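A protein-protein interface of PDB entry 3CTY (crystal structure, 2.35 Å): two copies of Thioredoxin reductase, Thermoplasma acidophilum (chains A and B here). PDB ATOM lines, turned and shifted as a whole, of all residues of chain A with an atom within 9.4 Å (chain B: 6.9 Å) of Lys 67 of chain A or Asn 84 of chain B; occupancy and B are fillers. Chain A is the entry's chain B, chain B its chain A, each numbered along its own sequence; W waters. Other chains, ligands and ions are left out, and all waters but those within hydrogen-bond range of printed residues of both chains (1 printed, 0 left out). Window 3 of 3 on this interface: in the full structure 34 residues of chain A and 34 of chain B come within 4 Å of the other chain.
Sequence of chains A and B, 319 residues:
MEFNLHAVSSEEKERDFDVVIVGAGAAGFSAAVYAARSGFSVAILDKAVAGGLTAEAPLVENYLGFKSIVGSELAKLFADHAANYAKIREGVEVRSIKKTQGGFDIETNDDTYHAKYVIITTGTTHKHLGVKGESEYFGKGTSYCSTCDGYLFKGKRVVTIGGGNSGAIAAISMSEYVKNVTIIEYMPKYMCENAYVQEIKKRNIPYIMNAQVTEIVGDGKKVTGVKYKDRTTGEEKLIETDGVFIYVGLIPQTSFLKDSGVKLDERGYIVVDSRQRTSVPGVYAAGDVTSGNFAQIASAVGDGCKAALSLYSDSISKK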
ATOM      1  N   LEU A  59      21.362 -25.198  29.554  1.00  0.00           N
ATOM      2  CA  LEU A  59      22.396 -24.166  29.598  1.00  0.00           C
ATOM      3  C   LEU A  59      22.288 -23.160  28.454  1.00  0.00           C
ATOM      4  O   LEU A  59      22.550 -23.493  27.303  1.00  0.00           O
ATOM      5  CB  LEU A  59      23.779 -24.823  29.574  1.00  0.00           C
ATOM      6  CG  LEU A  59      24.947 -23.934  29.999  1.00  0.00           C
ATOM      7  CD1 LEU A  59      24.711 -23.421  31.414  1.00  0.00           C
ATOM      8  CD2 LEU A  59      26.238 -24.719  29.933  1.00  0.00           C
ATOM      9  N   VAL A  60      21.923 -21.925  28.789  1.00  0.00           N
ATOM     10  CA  VAL A  60      21.762 -20.853  27.806  1.00  0.00           C
ATOM     11  C   VAL A  60      23.025 -20.007  27.652  1.00  0.00           C
ATOM     12  O   VAL A  60      23.428 -19.315  28.585  1.00  0.00           O
ATOM     13  CB  VAL A  60      20.599 -19.920  28.205  1.00  0.00           C
ATOM     14  CG1 VAL A  60      20.410 -18.836  27.150  1.00  0.00           C
ATOM     15  CG2 VAL A  60      19.331 -20.732  28.379  1.00  0.00           C
ATOM     16  N   GLU A  61      23.637 -20.052  26.470  1.00  0.00           N
ATOM     17  CA  GLU A  61      24.859 -19.280  26.228  1.00  0.00           C
ATOM     18  C   GLU A  61      24.746 -18.339  25.037  1.00  0.00           C
ATOM     19  O   GLU A  61      25.750 -17.770  24.603  1.00  0.00           O
ATOM     20  CB  GLU A  61      26.041 -20.212  25.975  1.00  0.00           C
ATOM     21  CG  GLU A  61      25.930 -21.556  26.656  1.00  0.00           C
ATOM     22  CD  GLU A  61      27.115 -22.449  26.351  1.00  0.00           C
ATOM     23  OE1 GLU A  61      28.202 -22.193  26.915  1.00  0.00           O
ATOM     24  OE2 GLU A  61      26.954 -23.394  25.541  1.00  0.00           O
ATOM     25  N   ASN A  62      23.540 -18.179  24.497  1.00  0.00           N
ATOM     26  CA  ASN A  62      23.373 -17.305  23.354  1.00  0.00           C
ATOM     27  C   ASN A  62      22.404 -16.138  23.581  1.00  0.00           C
ATOM     28  O   ASN A  62      21.854 -15.595  22.630  1.00  0.00           O
ATOM     29  CB  ASN A  62      22.950 -18.114  22.131  1.00  0.00           C
ATOM     30  CG  ASN A  62      21.713 -18.956  22.385  1.00  0.00           C
ATOM     31  OD1 ASN A  62      20.945 -18.697  23.314  1.00  0.00           O
ATOM     32  ND2 ASN A  62      21.506 -19.954  21.549  1.00  0.00           N
ATOM     33  N   TYR A  63      22.181 -15.777  24.844  1.00  0.00           N
ATOM     34  CA  TYR A  63      21.321 -14.642  25.175  1.00  0.00           C
ATOM     35  C   TYR A  63      22.294 -13.555  25.632  1.00  0.00           C
ATOM     36  O   TYR A  63      22.808 -13.611  26.744  1.00  0.00           O
ATOM     37  CB  TYR A  63      20.366 -14.988  26.306  1.00  0.00           C
ATOM     38  CG  TYR A  63      19.506 -13.817  26.724  1.00  0.00           C
ATOM     39  CD1 TYR A  63      18.666 -13.189  25.812  1.00  0.00           C
ATOM     40  CD2 TYR A  63      19.553 -13.323  28.029  1.00  0.00           C
ATOM     41  CE1 TYR A  63      17.889 -12.094  26.185  1.00  0.00           C
ATOM     42  CE2 TYR A  63      18.781 -12.220  28.411  1.00  0.00           C
ATOM     43  CZ  TYR A  63      17.952 -11.612  27.485  1.00  0.00           C
ATOM     44  OH  TYR A  63      17.188 -10.528  27.856  1.00  0.00           O
ATOM     45  N   LEU A  64      22.544 -12.586  24.760  1.00  0.00           N
ATOM     46  CA  LEU A  64      23.507 -11.511  25.022  1.00  0.00           C
ATOM     47  C   LEU A  64      23.548 -10.927  26.424  1.00  0.00           C
ATOM     48  O   LEU A  64      22.585 -10.306  26.876  1.00  0.00           O
ATOM     49  CB  LEU A  64      23.302 -10.364  24.034  1.00  0.00           C
ATOM     50  CG  LEU A  64      24.513  -9.944  23.195  1.00  0.00           C
ATOM     51  CD1 LEU A  64      24.501  -8.421  23.050  1.00  0.00           C
ATOM     52  CD2 LEU A  64      25.812 -10.416  23.830  1.00  0.00           C
ATOM     53  N   GLY A  65      24.681 -11.100  27.099  1.00  0.00           N
ATOM     54  CA  GLY A  65      24.819 -10.570  28.446  1.00  0.00           C
ATOM     55  C   GLY A  65      25.162 -11.639  29.464  1.00  0.00           C
ATOM     56  O   GLY A  65      25.729 -11.350  30.516  1.00  0.00           O
ATOM     57  N   PHE A  66      24.798 -12.880  29.165  1.00  0.00           N
ATOM     58  CA  PHE A  66      25.111 -13.993  30.062  1.00  0.00           C
ATOM     59  C   PHE A  66      25.934 -14.987  29.247  1.00  0.00           C
ATOM     60  O   PHE A  66      25.395 -15.667  28.370  1.00  0.00           O
ATOM     61  CB  PHE A  66      23.832 -14.679  30.572  1.00  0.00           C
ATOM     62  CG  PHE A  66      22.907 -13.773  31.349  1.00  0.00           C
ATOM     63  CD1 PHE A  66      21.997 -12.950  30.691  1.00  0.00           C
ATOM     64  CD2 PHE A  66      22.942 -13.748  32.742  1.00  0.00           C
ATOM     65  CE1 PHE A  66      21.127 -12.112  31.407  1.00  0.00           C
ATOM     66  CE2 PHE A  66      22.077 -12.913  33.475  1.00  0.00           C
ATOM     67  CZ  PHE A  66      21.166 -12.093  32.801  1.00  0.00           C
ATOM     68  N   LYS A  67      27.238 -15.050  29.508  1.00  0.00           N
ATOM     69  CA  LYS A  67      28.105 -15.971  28.777  1.00  0.00           C
ATOM     70  C   LYS A  67      27.538 -17.381  28.879  1.00  0.00           C
ATOM     71  O   LYS A  67      27.398 -18.078  27.873  1.00  0.00           O
ATOM     72  CB  LYS A  67      29.527 -15.934  29.336  1.00  0.00           C
ATOM     73  CG  LYS A  67      30.239 -14.620  29.098  1.00  0.00           C
ATOM     74  CD  LYS A  67      31.674 -14.627  29.621  1.00  0.00           C
ATOM     75  CE  LYS A  67      32.355 -13.283  29.338  1.00  0.00           C
ATOM     76  NZ  LYS A  67      33.810 -13.252  29.679  1.00  0.00           N
ATOM     77  N   SER A  68      27.205 -17.797  30.095  1.00  0.00           N
ATOM     78  CA  SER A  68      26.634 -19.121  30.312  1.00  0.00           C
ATOM     79  C   SER A  68      25.786 -19.093  31.568  1.00  0.00           C
ATOM     80  O   SER A  68      26.231 -18.635  32.617  1.00  0.00           O
ATOM     81  CB  SER A  68      27.739 -20.168  30.447  1.00  0.00           C
ATOM     82  OG  SER A  68      27.200 -21.479  30.466  1.00  0.00           O
ATOM     83  N   ILE A  69      24.556 -19.575  31.463  1.00  0.00           N
ATOM     84  CA  ILE A  69      23.662 -19.573  32.611  1.00  0.00           C
ATOM     85  C   ILE A  69      22.588 -20.652  32.516  1.00  0.00           C
ATOM     86  O   ILE A  69      21.950 -20.832  31.473  1.00  0.00           O
ATOM     87  CB  ILE A  69      22.991 -18.177  32.778  1.00  0.00           C
ATOM     88  CG1 ILE A  69      22.046 -18.190  33.985  1.00  0.00           C
ATOM     89  CG2 ILE A  69      22.269 -17.786  31.483  1.00  0.00           C
ATOM     90  CD1 ILE A  69      21.569 -16.816  34.419  1.00  0.00           C
ATOM     91  N   VAL A  70      22.400 -21.380  33.610  1.00  0.00           N
ATOM     92  CA  VAL A  70      21.396 -22.431  33.647  1.00  0.00           C
ATOM     93  C   VAL A  70      20.018 -21.837  33.368  1.00  0.00           C
ATOM     94  O   VAL A  70      19.640 -20.818  33.948  1.00  0.00           O
ATOM     95  CB  VAL A  70      21.394 -23.119  35.015  1.00  0.00           C
ATOM     96  CG1 VAL A  70      20.306 -24.185  35.065  1.00  0.00           C
ATOM     97  CG2 VAL A  70      22.772 -23.719  35.277  1.00  0.00           C
ATOM     98  N   LEU A  74      18.040 -18.246  34.673  1.00  0.00           N
ATOM     99  CA  LEU A  74      17.655 -17.105  33.849  1.00  0.00           C
ATOM    100  C   LEU A  74      16.149 -16.834  33.970  1.00  0.00           C
ATOM    101  O   LEU A  74      15.730 -15.681  34.067  1.00  0.00           O
ATOM    102  CB  LEU A  74      18.038 -17.345  32.385  1.00  0.00           C
ATOM    103  CG  LEU A  74      17.812 -16.220  31.363  1.00  0.00           C
ATOM    104  CD1 LEU A  74      18.472 -14.925  31.809  1.00  0.00           C
ATOM    105  CD2 LEU A  74      18.390 -16.647  30.025  1.00  0.00           C
ATOM    106  N   ALA B  36      28.696 -17.342  15.005  1.00  0.00           N
ATOM    107  CA  ALA B  36      29.752 -18.255  15.399  1.00  0.00           C
ATOM    108  C   ALA B  36      29.165 -19.632  15.701  1.00  0.00           C
ATOM    109  O   ALA B  36      29.520 -20.621  15.058  1.00  0.00           O
ATOM    110  CB  ALA B  36      30.471 -17.712  16.620  1.00  0.00           C
ATOM    111  N   ARG B  37      28.262 -19.690  16.679  1.00  0.00           N
ATOM    112  CA  ARG B  37      27.633 -20.950  17.067  1.00  0.00           C
ATOM    113  C   ARG B  37      27.032 -21.695  15.873  1.00  0.00           C
ATOM    114  O   ARG B  37      26.883 -22.920  15.908  1.00  0.00           O
ATOM    115  CB  ARG B  37      26.575 -20.698  18.147  1.00  0.00           C
ATOM    116  CG  ARG B  37      27.163 -20.155  19.456  1.00  0.00           C
ATOM    117  CD  ARG B  37      26.077 -19.949  20.487  1.00  0.00           C
ATOM    118  NE  ARG B  37      25.429 -21.208  20.833  1.00  0.00           N
ATOM    119  CZ  ARG B  37      25.940 -22.106  21.670  1.00  0.00           C
ATOM    120  NH1 ARG B  37      27.103 -21.880  22.255  1.00  0.00           N
ATOM    121  NH2 ARG B  37      25.286 -23.234  21.918  1.00  0.00           N
ATOM    122  N   LYS B  76      29.784  -3.673  28.449  1.00  0.00           N
ATOM    123  CA  LYS B  76      30.990  -4.424  28.780  1.00  0.00           C
ATOM    124  C   LYS B  76      30.668  -5.921  28.755  1.00  0.00           C
ATOM    125  O   LYS B  76      31.406  -6.718  28.178  1.00  0.00           O
ATOM    126  CB  LYS B  76      31.487  -4.012  30.170  1.00  0.00           C
ATOM    127  CG  LYS B  76      32.769  -4.685  30.619  1.00  0.00           C
ATOM    128  CD  LYS B  76      33.156  -4.229  32.032  1.00  0.00           C
ATOM    129  CE  LYS B  76      34.425  -4.930  32.534  1.00  0.00           C
ATOM    130  NZ  LYS B  76      34.304  -6.421  32.476  1.00  0.00           N
ATOM    131  N   LEU B  77      29.549  -6.291  29.370  1.00  0.00           N
ATOM    132  CA  LEU B  77      29.126  -7.685  29.405  1.00  0.00           C
ATOM    133  C   LEU B  77      28.826  -8.165  27.993  1.00  0.00           C
ATOM    134  O   LEU B  77      29.187  -9.284  27.630  1.00  0.00           O
ATOM    135  CB  LEU B  77      27.887  -7.846  30.287  1.00  0.00           C
ATOM    136  CG  LEU B  77      28.058  -7.485  31.770  1.00  0.00           C
ATOM    137  CD1 LEU B  77      26.693  -7.467  32.453  1.00  0.00           C
ATOM    138  CD2 LEU B  77      28.995  -8.484  32.442  1.00  0.00           C
ATOM    139  N   ALA B  79      30.062  -7.058  25.025  1.00  0.00           N
ATOM    140  CA  ALA B  79      31.323  -7.234  24.318  1.00  0.00           C
ATOM    141  C   ALA B  79      32.108  -8.464  24.781  1.00  0.00           C
ATOM    142  O   ALA B  79      32.604  -9.232  23.951  1.00  0.00           O
ATOM    143  CB  ALA B  79      32.174  -5.981  24.460  1.00  0.00           C
ATOM    144  N   ASP B  80      32.213  -8.661  26.094  1.00  0.00           N
ATOM    145  CA  ASP B  80      32.960  -9.808  26.616  1.00  0.00           C
ATOM    146  C   ASP B  80      32.331 -11.130  26.201  1.00  0.00           C
ATOM    147  O   ASP B  80      33.031 -12.128  25.989  1.00  0.00           O
ATOM    148  CB  ASP B  80      33.063  -9.748  28.146  1.00  0.00           C
ATOM    149  CG  ASP B  80      33.852  -8.541  28.631  1.00  0.00           C
ATOM    150  OD1 ASP B  80      34.717  -8.052  27.867  1.00  0.00           O
ATOM    151  OD2 ASP B  80      33.620  -8.090  29.779  1.00  0.00           O
ATOM    152  N   HIS B  81      31.006 -11.124  26.086  1.00  0.00           N
ATOM    153  CA  HIS B  81      30.260 -12.305  25.692  1.00  0.00           C
ATOM    154  C   HIS B  81      30.549 -12.582  24.224  1.00  0.00           C
ATOM    155  O   HIS B  81      30.849 -13.711  23.839  1.00  0.00           O
ATOM    156  CB  HIS B  81      28.756 -12.064  25.893  1.00  0.00           C
ATOM    157  CG  HIS B  81      27.905 -13.270  25.645  1.00  0.00           C
ATOM    158  ND1 HIS B  81      26.530 -13.241  25.742  1.00  0.00           N
ATOM    159  CD2 HIS B  81      28.232 -14.542  25.312  1.00  0.00           C
ATOM    160  CE1 HIS B  81      26.048 -14.443  25.479  1.00  0.00           C
ATOM    161  NE2 HIS B  81      27.061 -15.250  25.215  1.00  0.00           N
ATOM    162  N   ALA B  82      30.458 -11.537  23.409  1.00  0.00           N
ATOM    163  CA  ALA B  82      30.689 -11.665  21.981  1.00  0.00           C
ATOM    164  C   ALA B  82      32.140 -12.018  21.691  1.00  0.00           C
ATOM    165  O   ALA B  82      32.431 -12.737  20.739  1.00  0.00           O
ATOM    166  CB  ALA B  82      30.310 -10.374  21.282  1.00  0.00           C
ATOM    167  N   ALA B  83      33.043 -11.517  22.530  1.00  0.00           N
ATOM    168  CA  ALA B  83      34.476 -11.760  22.369  1.00  0.00           C
ATOM    169  C   ALA B  83      34.833 -13.238  22.247  1.00  0.00           C
ATOM    170  O   ALA B  83      35.773 -13.594  21.538  1.00  0.00           O
ATOM    171  CB  ALA B  83      35.249 -11.134  23.540  1.00  0.00           C
ATOM    172  N   ASN B  84      34.079 -14.090  22.935  1.00  0.00           N
ATOM    173  CA  ASN B  84      34.324 -15.529  22.914  1.00  0.00           C
ATOM    174  C   ASN B  84      33.913 -16.206  21.609  1.00  0.00           C
ATOM    175  O   ASN B  84      34.106 -17.406  21.449  1.00  0.00           O
ATOM    176  CB  ASN B  84      33.582 -16.231  24.066  1.00  0.00           C
ATOM    177  CG  ASN B  84      34.158 -15.904  25.439  1.00  0.00           C
ATOM    178  OD1 ASN B  84      35.374 -15.800  25.610  1.00  0.00           O
ATOM    179  ND2 ASN B  84      33.282 -15.769  26.431  1.00  0.00           N
ATOM    180  N   TYR B  85      33.354 -15.451  20.672  1.00  0.00           N
ATOM    181  CA  TYR B  85      32.909 -16.055  19.424  1.00  0.00           C
ATOM    182  C   TYR B  85      33.353 -15.330  18.169  1.00  0.00           C
ATOM    183  O   TYR B  85      33.247 -15.874  17.067  1.00  0.00           O
ATOM    184  CB  TYR B  85      31.382 -16.155  19.395  1.00  0.00           C
ATOM    185  CG  TYR B  85      30.766 -16.906  20.548  1.00  0.00           C
ATOM    186  CD1 TYR B  85      30.524 -16.274  21.768  1.00  0.00           C
ATOM    187  CD2 TYR B  85      30.388 -18.239  20.408  1.00  0.00           C
ATOM    188  CE1 TYR B  85      29.907 -16.953  22.824  1.00  0.00           C
ATOM    189  CE2 TYR B  85      29.778 -18.929  21.453  1.00  0.00           C
ATOM    190  CZ  TYR B  85      29.538 -18.282  22.657  1.00  0.00           C
ATOM    191  OH  TYR B  85      28.921 -18.961  23.682  1.00  0.00           O
ATOM    192  N   ALA B  86      33.832 -14.103  18.319  1.00  0.00           N
ATOM    193  CA  ALA B  86      34.254 -13.343  17.151  1.00  0.00           C
ATOM    194  C   ALA B  86      35.444 -12.447  17.429  1.00  0.00           C
ATOM    195  O   ALA B  86      35.783 -12.175  18.583  1.00  0.00           O
ATOM    196  CB  ALA B  86      33.085 -12.503  16.630  1.00  0.00           C
ATOM    197  N   ILE B  88      36.888  -8.907  17.479  1.00  0.00           N
ATOM    198  CA  ILE B  88      36.386  -7.537  17.511  1.00  0.00           C
ATOM    199  C   ILE B  88      37.495  -6.600  17.034  1.00  0.00           C
ATOM    200  O   ILE B  88      38.493  -6.422  17.721  1.00  0.00           O
ATOM    201  CB  ILE B  88      35.950  -7.130  18.940  1.00  0.00           C
ATOM    202  CG1 ILE B  88      34.993  -8.182  19.516  1.00  0.00           C
ATOM    203  CG2 ILE B  88      35.253  -5.779  18.903  1.00  0.00           C
ATOM    204  CD1 ILE B  88      34.710  -8.022  21.013  1.00  0.00           C
HETATM  205  O   HOH W   1      24.202 -24.252  25.082  1.00  0.00           O
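No position is printed for both chains.
Water W1 lies within hydrogen-bond range of the backbone carbonyl oxygen of Leu 59 of chain A (2.9 Å), the side-chain carboxylate of Glu 61 of chain A (2.9 Å) and the guanidinium group of Arg 37 of chain B (3.5 Å).
Of the printed residues of chain B, Lys 67 of chain A touches Asp 80 (3.6 Å), His 81 (3.8 Å) and Asn 84 (3.8 Å).
Asn 84 of chain B touches just one residue of chain A: Lys 67.
Of the printed residues of chain A, His 81 of chain B touches Glu 61, Tyr 63, Leu 64, Gly 65, Phe 66 and Lys 67.
No residue of chain A comes within 4 Å of Ala 83 of chain B.
Tyr 85 of chain B touches just one residue of chain A: Glu 61.
Printed residues of chain B within 4 Å of Asn 62 of chain A: Arg 37 (3.98 Å).
Of the printed residues of chain B, Glu 61 of chain A touches Arg 37 (3.6 Å), His 81 (2.9 Å) and Tyr 85 (3.5 Å).
Printed residues of chain A within 4 Å of Arg 37 of chain B: Glu 61 (3.6 Å) and Asn 62 (3.98 Å).
Of the printed residues of chain B, Phe 66 of chain A touches His 81.
Of the printed residues of chain B, Tyr 63 of chain A touches His 81 (3.6 Å).
Ala 36 of chain B touches none of the printed residues of chain A.
Val 60 of chain A touches none of the printed residues of chain B.
The nearest residue of chain A that does not touch Asn 84 of chain B is Ser 68 of chain A (7.4 Å).
A ring nitrogen (ND1) of His 81 of chain B lies within hydrogen-bond range of the backbone NH (N) of Gly 65 of chain A (3.1 Å).
The guanidinium group (NH1) of Arg 37 of chain B is in salt-bridge range of the side-chain carboxylate (OE2) of Glu 61 of chain A (3.6 Å).
A ring nitrogen (NE2) of His 81 of chain B lies within hydrogen-bond range of the backbone carbonyl oxygen (O) of Glu 61 of chain A, at 2.9 Å.
Of the 13 printed residues of chain A, 7 touch a printed residue of chain B.
Hydrophobic or aromatic side chains of chain B within 4 Å of the printed part of chain A: His 81 and Tyr 85.
The side-chain amino group (NZ) of Lys 76 of chain B is in salt-bridge range of the side-chain carboxylate (OD2) of Asp 80 of chain B, 3.2 Å away.
Among the printed residues, pairs that only touch across the chains: Glu 61 of chain A with Tyr 85 of chain B, Asn 62 of chain A with Arg 37 of chain B, Tyr 63 of chain A with His 81 of chain B, Leu 64 of chain A with His 81 of chain B, Phe 66 of chain A with His 81 of chain B, Lys 67 of chain A with Asp 80 of chain B, Lys 67 of chain A with His 81 of chain B and Lys 67 of chain A with Asn 84 of chain B.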
